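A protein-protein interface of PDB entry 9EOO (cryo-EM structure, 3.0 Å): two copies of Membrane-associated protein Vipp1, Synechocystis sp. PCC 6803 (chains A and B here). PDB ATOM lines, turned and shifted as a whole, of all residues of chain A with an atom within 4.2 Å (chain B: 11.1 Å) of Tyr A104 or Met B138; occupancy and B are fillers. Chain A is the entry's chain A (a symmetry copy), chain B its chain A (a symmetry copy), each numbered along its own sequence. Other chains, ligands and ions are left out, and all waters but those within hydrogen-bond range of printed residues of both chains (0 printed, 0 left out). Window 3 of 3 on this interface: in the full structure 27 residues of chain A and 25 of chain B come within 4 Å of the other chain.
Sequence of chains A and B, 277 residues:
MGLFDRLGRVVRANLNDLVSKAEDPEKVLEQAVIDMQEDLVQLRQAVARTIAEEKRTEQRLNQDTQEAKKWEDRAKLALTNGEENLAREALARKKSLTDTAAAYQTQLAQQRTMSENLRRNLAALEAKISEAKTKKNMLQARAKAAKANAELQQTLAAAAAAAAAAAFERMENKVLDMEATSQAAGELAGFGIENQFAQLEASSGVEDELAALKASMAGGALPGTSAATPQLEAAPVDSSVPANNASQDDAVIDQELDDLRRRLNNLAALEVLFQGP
Of the 11 printed residues of chain A, 4 touch a printed residue of chain B.
Hydrophobic or aromatic side chains of chain A within 4 Å of the printed part of chain B: Ala A103 and Tyr A104.
Of the 22 printed residues of chain B, 4 touch a printed residue of chain A.
Printed residues of chain B that touch a printed residue of chain A: Met B138, Ala B141, Arg B142 and Ala B145.
Hydrophobic or aromatic side chains of chain B that line the printed part of chain A: Met B138, Ala B141 and Ala B145.
Among the printed residues, 4 pairs touch across the chains.
Among the printed residues, no Asp or Glu carboxylate lies within 4 Å of a Lys or Arg side-chain nitrogen of the other chain.
No residue of chain B comes within 4 Å of Thr A100.
No residue of chain B comes within 4 Å of Ala A101.
Of chain B, only Arg B142 comes within 4 Å of Ala A103.
Of the printed residues of chain B, Tyr A104 touches Met B138 (3.3 Å).
No residue of chain B comes within 4 Å of Gln A105.
No residue of chain B comes within 4 Å of Thr A106.
Of the printed residues of chain B, Gln A107 touches Ala B145.
No residue of chain B comes within 4 Å of Leu A108.
Of chain A, only Tyr A104 (3.3 Å) comes within 4 Å of Met B138.
Of the printed residues of chain A, Ala B141 touches Arg A60.
Of the printed residues of chain A, Arg B142 touches Ala A103.
Of the printed residues of chain A, Ala B145 touches Gln A107.
The guanidinium group (NE) of Arg B142 is in hydrogen-bond range of the side-chain sulfur (SD) of Met B138 (3.5 Å).
No position is printed for both chains.
Of the 4 pairs that touch across the chains among the printed residues, none has its exchanged pair printed and touching as well.
Arg A60 touches Ala B141 (NE to CB, 3.9 Å).
Ala A103 touches Arg B142.
CA of Met B138 touches OH of Tyr A104, 3.3 Å away.
Ala B145 touches Gln A107.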
ATOM      1  N   ARG A  60      -5.632  18.346   1.131  1.00  0.00           N
ATOM      2  CA  ARG A  60      -6.770  18.732   1.955  1.00  0.00           C
ATOM      3  C   ARG A  60      -7.962  17.798   1.797  1.00  0.00           C
ATOM      4  O   ARG A  60      -8.655  17.489   2.773  1.00  0.00           O
ATOM      5  CB  ARG A  60      -7.189  20.145   1.590  1.00  0.00           C
ATOM      6  CG  ARG A  60      -6.166  21.202   1.868  1.00  0.00           C
ATOM      7  CD  ARG A  60      -6.694  22.530   1.412  1.00  0.00           C
ATOM      8  NE  ARG A  60      -5.651  23.457   1.000  1.00  0.00           N
ATOM      9  CZ  ARG A  60      -5.053  24.323   1.804  1.00  0.00           C
ATOM     10  NH1 ARG A  60      -5.270  24.317   3.111  1.00  0.00           N
ATOM     11  NH2 ARG A  60      -4.218  25.214   1.285  1.00  0.00           N
ATOM     12  N   ASP A  64     -10.042  15.588   4.996  1.00  0.00           N
ATOM     13  CA  ASP A  64     -11.451  15.712   5.338  1.00  0.00           C
ATOM     14  C   ASP A  64     -12.287  14.487   4.999  1.00  0.00           C
ATOM     15  O   ASP A  64     -13.377  14.334   5.558  1.00  0.00           O
ATOM     16  CB  ASP A  64     -12.042  16.925   4.631  1.00  0.00           C
ATOM     17  CG  ASP A  64     -11.503  18.228   5.166  1.00  0.00           C
ATOM     18  OD1 ASP A  64     -10.554  18.189   5.975  1.00  0.00           O
ATOM     19  OD2 ASP A  64     -12.032  19.291   4.786  1.00  0.00           O
ATOM     20  N   THR A 100     -17.779  20.255   2.411  1.00  0.00           N
ATOM     21  CA  THR A 100     -16.577  20.930   1.941  1.00  0.00           C
ATOM     22  C   THR A 100     -15.676  20.031   1.102  1.00  0.00           C
ATOM     23  O   THR A 100     -14.999  20.519   0.194  1.00  0.00           O
ATOM     24  CB  THR A 100     -15.810  21.494   3.138  1.00  0.00           C
ATOM     25  OG1 THR A 100     -15.466  20.432   4.033  1.00  0.00           O
ATOM     26  CG2 THR A 100     -16.630  22.513   3.876  1.00  0.00           C
ATOM     27  N   ALA A 101     -15.652  18.727   1.382  1.00  0.00           N
ATOM     28  CA  ALA A 101     -14.937  17.787   0.526  1.00  0.00           C
ATOM     29  C   ALA A 101     -15.468  17.767  -0.900  1.00  0.00           C
ATOM     30  O   ALA A 101     -14.697  17.577  -1.845  1.00  0.00           O
ATOM     31  CB  ALA A 101     -15.024  16.388   1.117  1.00  0.00           C
ATOM     32  N   ALA A 102     -16.768  17.961  -1.075  1.00  0.00           N
ATOM     33  CA  ALA A 102     -17.354  18.002  -2.409  1.00  0.00           C
ATOM     34  C   ALA A 102     -16.915  19.229  -3.189  1.00  0.00           C
ATOM     35  O   ALA A 102     -16.844  19.191  -4.422  1.00  0.00           O
ATOM     36  CB  ALA A 102     -18.868  17.970  -2.300  1.00  0.00           C
ATOM     37  N   ALA A 103     -16.619  20.321  -2.493  1.00  0.00           N
ATOM     38  CA  ALA A 103     -16.026  21.488  -3.129  1.00  0.00           C
ATOM     39  C   ALA A 103     -14.602  21.238  -3.606  1.00  0.00           C
ATOM     40  O   ALA A 103     -14.227  21.674  -4.700  1.00  0.00           O
ATOM     41  CB  ALA A 103     -16.045  22.658  -2.155  1.00  0.00           C
ATOM     42  N   TYR A 104     -13.792  20.548  -2.810  1.00  0.00           N
ATOM     43  CA  TYR A 104     -12.448  20.202  -3.260  1.00  0.00           C
ATOM     44  C   TYR A 104     -12.447  19.287  -4.480  1.00  0.00           C
ATOM     45  O   TYR A 104     -11.592  19.430  -5.361  1.00  0.00           O
ATOM     46  CB  TYR A 104     -11.676  19.537  -2.127  1.00  0.00           C
ATOM     47  CG  TYR A 104     -11.349  20.429  -0.960  1.00  0.00           C
ATOM     48  CD1 TYR A 104     -10.739  21.652  -1.147  1.00  0.00           C
ATOM     49  CD2 TYR A 104     -11.611  20.032   0.334  1.00  0.00           C
ATOM     50  CE1 TYR A 104     -10.434  22.463  -0.087  1.00  0.00           C
ATOM     51  CE2 TYR A 104     -11.300  20.830   1.399  1.00  0.00           C
ATOM     52  CZ  TYR A 104     -10.707  22.041   1.185  1.00  0.00           C
ATOM     53  OH  TYR A 104     -10.386  22.826   2.260  1.00  0.00           O
ATOM     54  N   GLN A 105     -13.381  18.343  -4.563  1.00  0.00           N
ATOM     55  CA  GLN A 105     -13.482  17.530  -5.770  1.00  0.00           C
ATOM     56  C   GLN A 105     -13.788  18.365  -7.004  1.00  0.00           C
ATOM     57  O   GLN A 105     -13.205  18.144  -8.072  1.00  0.00           O
ATOM     58  CB  GLN A 105     -14.547  16.461  -5.590  1.00  0.00           C
ATOM     59  CG  GLN A 105     -14.102  15.318  -4.732  1.00  0.00           C
ATOM     60  CD  GLN A 105     -13.186  14.372  -5.468  1.00  0.00           C
ATOM     61  OE1 GLN A 105     -12.592  14.730  -6.485  1.00  0.00           O
ATOM     62  NE2 GLN A 105     -13.057  13.158  -4.955  1.00  0.00           N
ATOM     63  N   THR A 106     -14.695  19.325  -6.882  1.00  0.00           N
ATOM     64  CA  THR A 106     -15.051  20.167  -8.017  1.00  0.00           C
ATOM     65  C   THR A 106     -13.903  21.077  -8.424  1.00  0.00           C
ATOM     66  O   THR A 106     -13.579  21.203  -9.612  1.00  0.00           O
ATOM     67  CB  THR A 106     -16.281  20.996  -7.664  1.00  0.00           C
ATOM     68  OG1 THR A 106     -17.369  20.124  -7.343  1.00  0.00           O
ATOM     69  CG2 THR A 106     -16.665  21.898  -8.803  1.00  0.00           C
ATOM     70  N   GLN A 107     -13.279  21.713  -7.445  1.00  0.00           N
ATOM     71  CA  GLN A 107     -12.105  22.544  -7.680  1.00  0.00           C
ATOM     72  C   GLN A 107     -10.980  21.764  -8.354  1.00  0.00           C
ATOM     73  O   GLN A 107     -10.390  22.231  -9.334  1.00  0.00           O
ATOM     74  CB  GLN A 107     -11.656  23.115  -6.339  1.00  0.00           C
ATOM     75  CG  GLN A 107     -10.450  23.995  -6.354  1.00  0.00           C
ATOM     76  CD  GLN A 107     -10.794  25.410  -6.741  1.00  0.00           C
ATOM     77  OE1 GLN A 107     -11.876  25.676  -7.267  1.00  0.00           O
ATOM     78  NE2 GLN A 107      -9.893  26.336  -6.454  1.00  0.00           N
ATOM     79  N   LEU A 108     -10.670  20.577  -7.843  1.00  0.00           N
ATOM     80  CA  LEU A 108      -9.509  19.831  -8.314  1.00  0.00           C
ATOM     81  C   LEU A 108      -9.649  19.334  -9.750  1.00  0.00           C
ATOM     82  O   LEU A 108      -8.685  19.383 -10.520  1.00  0.00           O
ATOM     83  CB  LEU A 108      -9.287  18.640  -7.392  1.00  0.00           C
ATOM     84  CG  LEU A 108      -8.118  17.719  -7.692  1.00  0.00           C
ATOM     85  CD1 LEU A 108      -6.822  18.481  -7.638  1.00  0.00           C
ATOM     86  CD2 LEU A 108      -8.113  16.579  -6.722  1.00  0.00           C
ATOM     87  N   PRO B  25      -9.945  39.903   2.713  1.00  0.00           N
ATOM     88  CA  PRO B  25     -10.589  38.633   3.073  1.00  0.00           C
ATOM     89  C   PRO B  25      -9.699  37.626   3.766  1.00  0.00           C
ATOM     90  O   PRO B  25     -10.198  36.807   4.545  1.00  0.00           O
ATOM     91  CB  PRO B  25     -11.064  38.097   1.718  1.00  0.00           C
ATOM     92  CG  PRO B  25     -11.251  39.280   0.900  1.00  0.00           C
ATOM     93  CD  PRO B  25     -10.177  40.235   1.302  1.00  0.00           C
ATOM     94  N   GLU B  26      -8.403  37.650   3.508  1.00  0.00           N
ATOM     95  CA  GLU B  26      -7.516  36.619   4.028  1.00  0.00           C
ATOM     96  C   GLU B  26      -7.135  36.867   5.480  1.00  0.00           C
ATOM     97  O   GLU B  26      -7.026  35.920   6.266  1.00  0.00           O
ATOM     98  CB  GLU B  26      -6.271  36.536   3.151  1.00  0.00           C
ATOM     99  CG  GLU B  26      -5.453  35.289   3.365  1.00  0.00           C
ATOM    100  CD  GLU B  26      -4.288  35.189   2.403  1.00  0.00           C
ATOM    101  OE1 GLU B  26      -4.508  35.354   1.184  1.00  0.00           O
ATOM    102  OE2 GLU B  26      -3.151  34.952   2.864  1.00  0.00           O
ATOM    103  N   LEU B  29     -10.698  37.202   7.937  1.00  0.00           N
ATOM    104  CA  LEU B  29     -11.497  35.998   8.080  1.00  0.00           C
ATOM    105  C   LEU B  29     -11.004  35.087   9.199  1.00  0.00           C
ATOM    106  O   LEU B  29     -11.805  34.352   9.786  1.00  0.00           O
ATOM    107  CB  LEU B  29     -11.490  35.267   6.745  1.00  0.00           C
ATOM    108  CG  LEU B  29     -12.394  34.077   6.521  1.00  0.00           C
ATOM    109  CD1 LEU B  29     -13.812  34.529   6.552  1.00  0.00           C
ATOM    110  CD2 LEU B  29     -12.078  33.485   5.183  1.00  0.00           C
ATOM    111  N   GLU B  30      -9.713  35.109   9.507  1.00  0.00           N
ATOM    112  CA  GLU B  30      -9.189  34.394  10.664  1.00  0.00           C
ATOM    113  C   GLU B  30      -9.238  35.174  11.972  1.00  0.00           C
ATOM    114  O   GLU B  30      -9.395  34.569  13.037  1.00  0.00           O
ATOM    115  CB  GLU B  30      -7.737  34.001  10.415  1.00  0.00           C
ATOM    116  CG  GLU B  30      -6.825  35.182  10.258  1.00  0.00           C
ATOM    117  CD  GLU B  30      -5.465  34.801   9.720  1.00  0.00           C
ATOM    118  OE1 GLU B  30      -5.357  33.734   9.086  1.00  0.00           O
ATOM    119  OE2 GLU B  30      -4.503  35.572   9.930  1.00  0.00           O
ATOM    120  N   VAL B  33     -12.607  34.619  13.632  1.00  0.00           N
ATOM    121  CA  VAL B  33     -12.697  33.398  14.423  1.00  0.00           C
ATOM    122  C   VAL B  33     -11.970  33.519  15.754  1.00  0.00           C
ATOM    123  O   VAL B  33     -12.414  32.963  16.761  1.00  0.00           O
ATOM    124  CB  VAL B  33     -12.152  32.224  13.600  1.00  0.00           C
ATOM    125  CG1 VAL B  33     -12.270  30.948  14.372  1.00  0.00           C
ATOM    126  CG2 VAL B  33     -12.889  32.116  12.307  1.00  0.00           C
ATOM    127  N   SER B 130     -16.865  25.691  15.438  1.00  0.00           N
ATOM    128  CA  SER B 130     -16.236  24.552  14.781  1.00  0.00           C
ATOM    129  C   SER B 130     -16.527  24.528  13.287  1.00  0.00           C
ATOM    130  O   SER B 130     -15.628  24.281  12.474  1.00  0.00           O
ATOM    131  CB  SER B 130     -16.716  23.262  15.438  1.00  0.00           C
ATOM    132  OG  SER B 130     -16.000  22.142  14.966  1.00  0.00           O
ATOM    133  N   GLU B 131     -17.776  24.777  12.907  1.00  0.00           N
ATOM    134  CA  GLU B 131     -18.132  24.905  11.497  1.00  0.00           C
ATOM    135  C   GLU B 131     -17.406  26.056  10.813  1.00  0.00           C
ATOM    136  O   GLU B 131     -16.875  25.899   9.709  1.00  0.00           O
ATOM    137  CB  GLU B 131     -19.639  25.097  11.384  1.00  0.00           C
ATOM    138  CG  GLU B 131     -20.152  25.158   9.971  1.00  0.00           C
ATOM    139  CD  GLU B 131     -21.615  25.530   9.909  1.00  0.00           C
ATOM    140  OE1 GLU B 131     -22.315  25.361  10.930  1.00  0.00           O
ATOM    141  OE2 GLU B 131     -22.072  25.989   8.841  1.00  0.00           O
ATOM    142  N   ALA B 132     -17.384  27.224  11.441  1.00  0.00           N
ATOM    143  CA  ALA B 132     -16.679  28.363  10.864  1.00  0.00           C
ATOM    144  C   ALA B 132     -15.209  28.070  10.609  1.00  0.00           C
ATOM    145  O   ALA B 132     -14.664  28.448   9.566  1.00  0.00           O
ATOM    146  CB  ALA B 132     -16.807  29.565  11.787  1.00  0.00           C
ATOM    147  N   LYS B 133     -14.553  27.401  11.545  1.00  0.00           N
ATOM    148  CA  LYS B 133     -13.131  27.122  11.416  1.00  0.00           C
ATOM    149  C   LYS B 133     -12.809  26.122  10.315  1.00  0.00           C
ATOM    150  O   LYS B 133     -11.741  26.207   9.703  1.00  0.00           O
ATOM    151  CB  LYS B 133     -12.614  26.630  12.756  1.00  0.00           C
ATOM    152  CG  LYS B 133     -11.127  26.571  12.874  1.00  0.00           C
ATOM    153  CD  LYS B 133     -10.718  26.712  14.319  1.00  0.00           C
ATOM    154  CE  LYS B 133     -11.457  25.742  15.206  1.00  0.00           C
ATOM    155  NZ  LYS B 133     -10.960  25.793  16.595  1.00  0.00           N
ATOM    156  N   THR B 134     -13.700  25.174  10.051  1.00  0.00           N
ATOM    157  CA  THR B 134     -13.502  24.271   8.922  1.00  0.00           C
ATOM    158  C   THR B 134     -13.683  24.982   7.583  1.00  0.00           C
ATOM    159  O   THR B 134     -12.943  24.713   6.631  1.00  0.00           O
ATOM    160  CB  THR B 134     -14.445  23.074   9.056  1.00  0.00           C
ATOM    161  OG1 THR B 134     -14.111  22.092   8.072  1.00  0.00           O
ATOM    162  CG2 THR B 134     -15.871  23.461   8.854  1.00  0.00           C
ATOM    163  N   LYS B 135     -14.657  25.884   7.484  1.00  0.00           N
ATOM    164  CA  LYS B 135     -14.868  26.631   6.248  1.00  0.00           C
ATOM    165  C   LYS B 135     -13.749  27.622   5.965  1.00  0.00           C
ATOM    166  O   LYS B 135     -13.372  27.825   4.808  1.00  0.00           O
ATOM    167  CB  LYS B 135     -16.190  27.377   6.316  1.00  0.00           C
ATOM    168  CG  LYS B 135     -17.388  26.516   6.101  1.00  0.00           C
ATOM    169  CD  LYS B 135     -18.648  27.327   6.241  1.00  0.00           C
ATOM    170  CE  LYS B 135     -19.864  26.503   5.895  1.00  0.00           C
ATOM    171  NZ  LYS B 135     -21.121  27.233   6.183  1.00  0.00           N
ATOM    172  N   LYS B 136     -13.214  28.248   7.005  1.00  0.00           N
ATOM    173  CA  LYS B 136     -12.096  29.167   6.840  1.00  0.00           C
ATOM    174  C   LYS B 136     -10.966  28.550   6.032  1.00  0.00           C
ATOM    175  O   LYS B 136     -10.386  29.205   5.159  1.00  0.00           O
ATOM    176  CB  LYS B 136     -11.615  29.605   8.218  1.00  0.00           C
ATOM    177  CG  LYS B 136     -10.503  30.604   8.221  1.00  0.00           C
ATOM    178  CD  LYS B 136      -9.881  30.725   9.594  1.00  0.00           C
ATOM    179  CE  LYS B 136      -9.017  29.545   9.960  1.00  0.00           C
ATOM    180  NZ  LYS B 136      -7.691  29.614   9.312  1.00  0.00           N
ATOM    181  N   ASN B 137     -10.627  27.300   6.318  1.00  0.00           N
ATOM    182  CA  ASN B 137      -9.546  26.631   5.604  1.00  0.00           C
ATOM    183  C   ASN B 137      -9.841  26.515   4.111  1.00  0.00           C
ATOM    184  O   ASN B 137      -8.979  26.792   3.271  1.00  0.00           O
ATOM    185  CB  ASN B 137      -9.339  25.250   6.212  1.00  0.00           C
ATOM    186  CG  ASN B 137      -8.757  25.314   7.598  1.00  0.00           C
ATOM    187  OD1 ASN B 137      -8.265  26.354   8.032  1.00  0.00           O
ATOM    188  ND2 ASN B 137      -8.839  24.209   8.317  1.00  0.00           N
ATOM    189  N   MET B 138     -11.058  26.107   3.768  1.00  0.00           N
ATOM    190  CA  MET B 138     -11.456  25.950   2.373  1.00  0.00           C
ATOM    191  C   MET B 138     -11.514  27.273   1.623  1.00  0.00           C
ATOM    192  O   MET B 138     -11.187  27.332   0.434  1.00  0.00           O
ATOM    193  CB  MET B 138     -12.815  25.266   2.307  1.00  0.00           C
ATOM    194  CG  MET B 138     -13.373  25.140   0.913  1.00  0.00           C
ATOM    195  SD  MET B 138     -14.381  26.534   0.388  1.00  0.00           S
ATOM    196  CE  MET B 138     -15.746  26.407   1.529  1.00  0.00           C
ATOM    197  N   LEU B 139     -11.930  28.343   2.290  1.00  0.00           N
ATOM    198  CA  LEU B 139     -11.983  29.651   1.650  1.00  0.00           C
ATOM    199  C   LEU B 139     -10.607  30.257   1.436  1.00  0.00           C
ATOM    200  O   LEU B 139     -10.338  30.831   0.375  1.00  0.00           O
ATOM    201  CB  LEU B 139     -12.834  30.591   2.488  1.00  0.00           C
ATOM    202  CG  LEU B 139     -14.318  30.269   2.563  1.00  0.00           C
ATOM    203  CD1 LEU B 139     -14.959  31.171   3.567  1.00  0.00           C
ATOM    204  CD2 LEU B 139     -14.993  30.409   1.229  1.00  0.00           C
ATOM    205  N   GLN B 140      -9.723  30.151   2.419  1.00  0.00           N
ATOM    206  CA  GLN B 140      -8.366  30.654   2.249  1.00  0.00           C
ATOM    207  C   GLN B 140      -7.617  29.927   1.144  1.00  0.00           C
ATOM    208  O   GLN B 140      -6.721  30.505   0.523  1.00  0.00           O
ATOM    209  CB  GLN B 140      -7.618  30.513   3.565  1.00  0.00           C
ATOM    210  CG  GLN B 140      -8.039  31.502   4.611  1.00  0.00           C
ATOM    211  CD  GLN B 140      -7.235  31.385   5.878  1.00  0.00           C
ATOM    212  OE1 GLN B 140      -6.958  30.285   6.352  1.00  0.00           O
ATOM    213  NE2 GLN B 140      -6.860  32.519   6.441  1.00  0.00           N
ATOM    214  N   ALA B 141      -7.961  28.672   0.888  1.00  0.00           N
ATOM    215  CA  ALA B 141      -7.414  27.960  -0.259  1.00  0.00           C
ATOM    216  C   ALA B 141      -7.887  28.535  -1.586  1.00  0.00           C
ATOM    217  O   ALA B 141      -7.080  28.841  -2.468  1.00  0.00           O
ATOM    218  CB  ALA B 141      -7.797  26.490  -0.165  1.00  0.00           C
ATOM    219  N   ARG B 142      -9.198  28.696  -1.737  1.00  0.00           N
ATOM    220  CA  ARG B 142      -9.777  29.284  -2.937  1.00  0.00           C
ATOM    221  C   ARG B 142      -9.287  30.693  -3.227  1.00  0.00           C
ATOM    222  O   ARG B 142      -9.149  31.069  -4.394  1.00  0.00           O
ATOM    223  CB  ARG B 142     -11.288  29.296  -2.790  1.00  0.00           C
ATOM    224  CG  ARG B 142     -11.934  27.957  -2.937  1.00  0.00           C
ATOM    225  CD  ARG B 142     -13.410  28.061  -2.685  1.00  0.00           C
ATOM    226  NE  ARG B 142     -14.116  26.856  -3.091  1.00  0.00           N
ATOM    227  CZ  ARG B 142     -15.368  26.835  -3.521  1.00  0.00           C
ATOM    228  NH1 ARG B 142     -16.083  27.940  -3.620  1.00  0.00           N
ATOM    229  NH2 ARG B 142     -15.909  25.679  -3.891  1.00  0.00           N
ATOM    230  N   ALA B 143      -9.025  31.489  -2.199  1.00  0.00           N
ATOM    231  CA  ALA B 143      -8.526  32.838  -2.424  1.00  0.00           C
ATOM    232  C   ALA B 143      -7.082  32.873  -2.904  1.00  0.00           C
ATOM    233  O   ALA B 143      -6.691  33.810  -3.606  1.00  0.00           O
ATOM    234  CB  ALA B 143      -8.654  33.649  -1.144  1.00  0.00           C
ATOM    235  N   LYS B 144      -6.278  31.886  -2.534  1.00  0.00           N
ATOM    236  CA  LYS B 144      -4.932  31.781  -3.085  1.00  0.00           C
ATOM    237  C   LYS B 144      -4.929  31.295  -4.528  1.00  0.00           C
ATOM    238  O   LYS B 144      -4.179  31.815  -5.360  1.00  0.00           O
ATOM    239  CB  LYS B 144      -4.105  30.851  -2.216  1.00  0.00           C
ATOM    240  CG  LYS B 144      -3.641  31.490  -0.929  1.00  0.00           C
ATOM    241  CD  LYS B 144      -3.030  30.483   0.028  1.00  0.00           C
ATOM    242  CE  LYS B 144      -1.889  29.703  -0.606  1.00  0.00           C
ATOM    243  NZ  LYS B 144      -0.729  30.580  -0.920  1.00  0.00           N
ATOM    244  N   ALA B 145      -5.750  30.300  -4.842  1.00  0.00           N
ATOM    245  CA  ALA B 145      -5.873  29.831  -6.216  1.00  0.00           C
ATOM    246  C   ALA B 145      -6.357  30.918  -7.162  1.00  0.00           C
ATOM    247  O   ALA B 145      -5.795  31.111  -8.244  1.00  0.00           O
ATOM    248  CB  ALA B 145      -6.810  28.633  -6.262  1.00  0.00           C
ATOM    249  N   ALA B 146      -7.400  31.642  -6.775  1.00  0.00           N
ATOM    250  CA  ALA B 146      -7.941  32.681  -7.640  1.00  0.00           C
ATOM    251  C   ALA B 146      -6.951  33.805  -7.896  1.00  0.00           C
ATOM    252  O   ALA B 146      -6.941  34.386  -8.985  1.00  0.00           O
ATOM    253  CB  ALA B 146      -9.203  33.251  -7.011  1.00  0.00           C
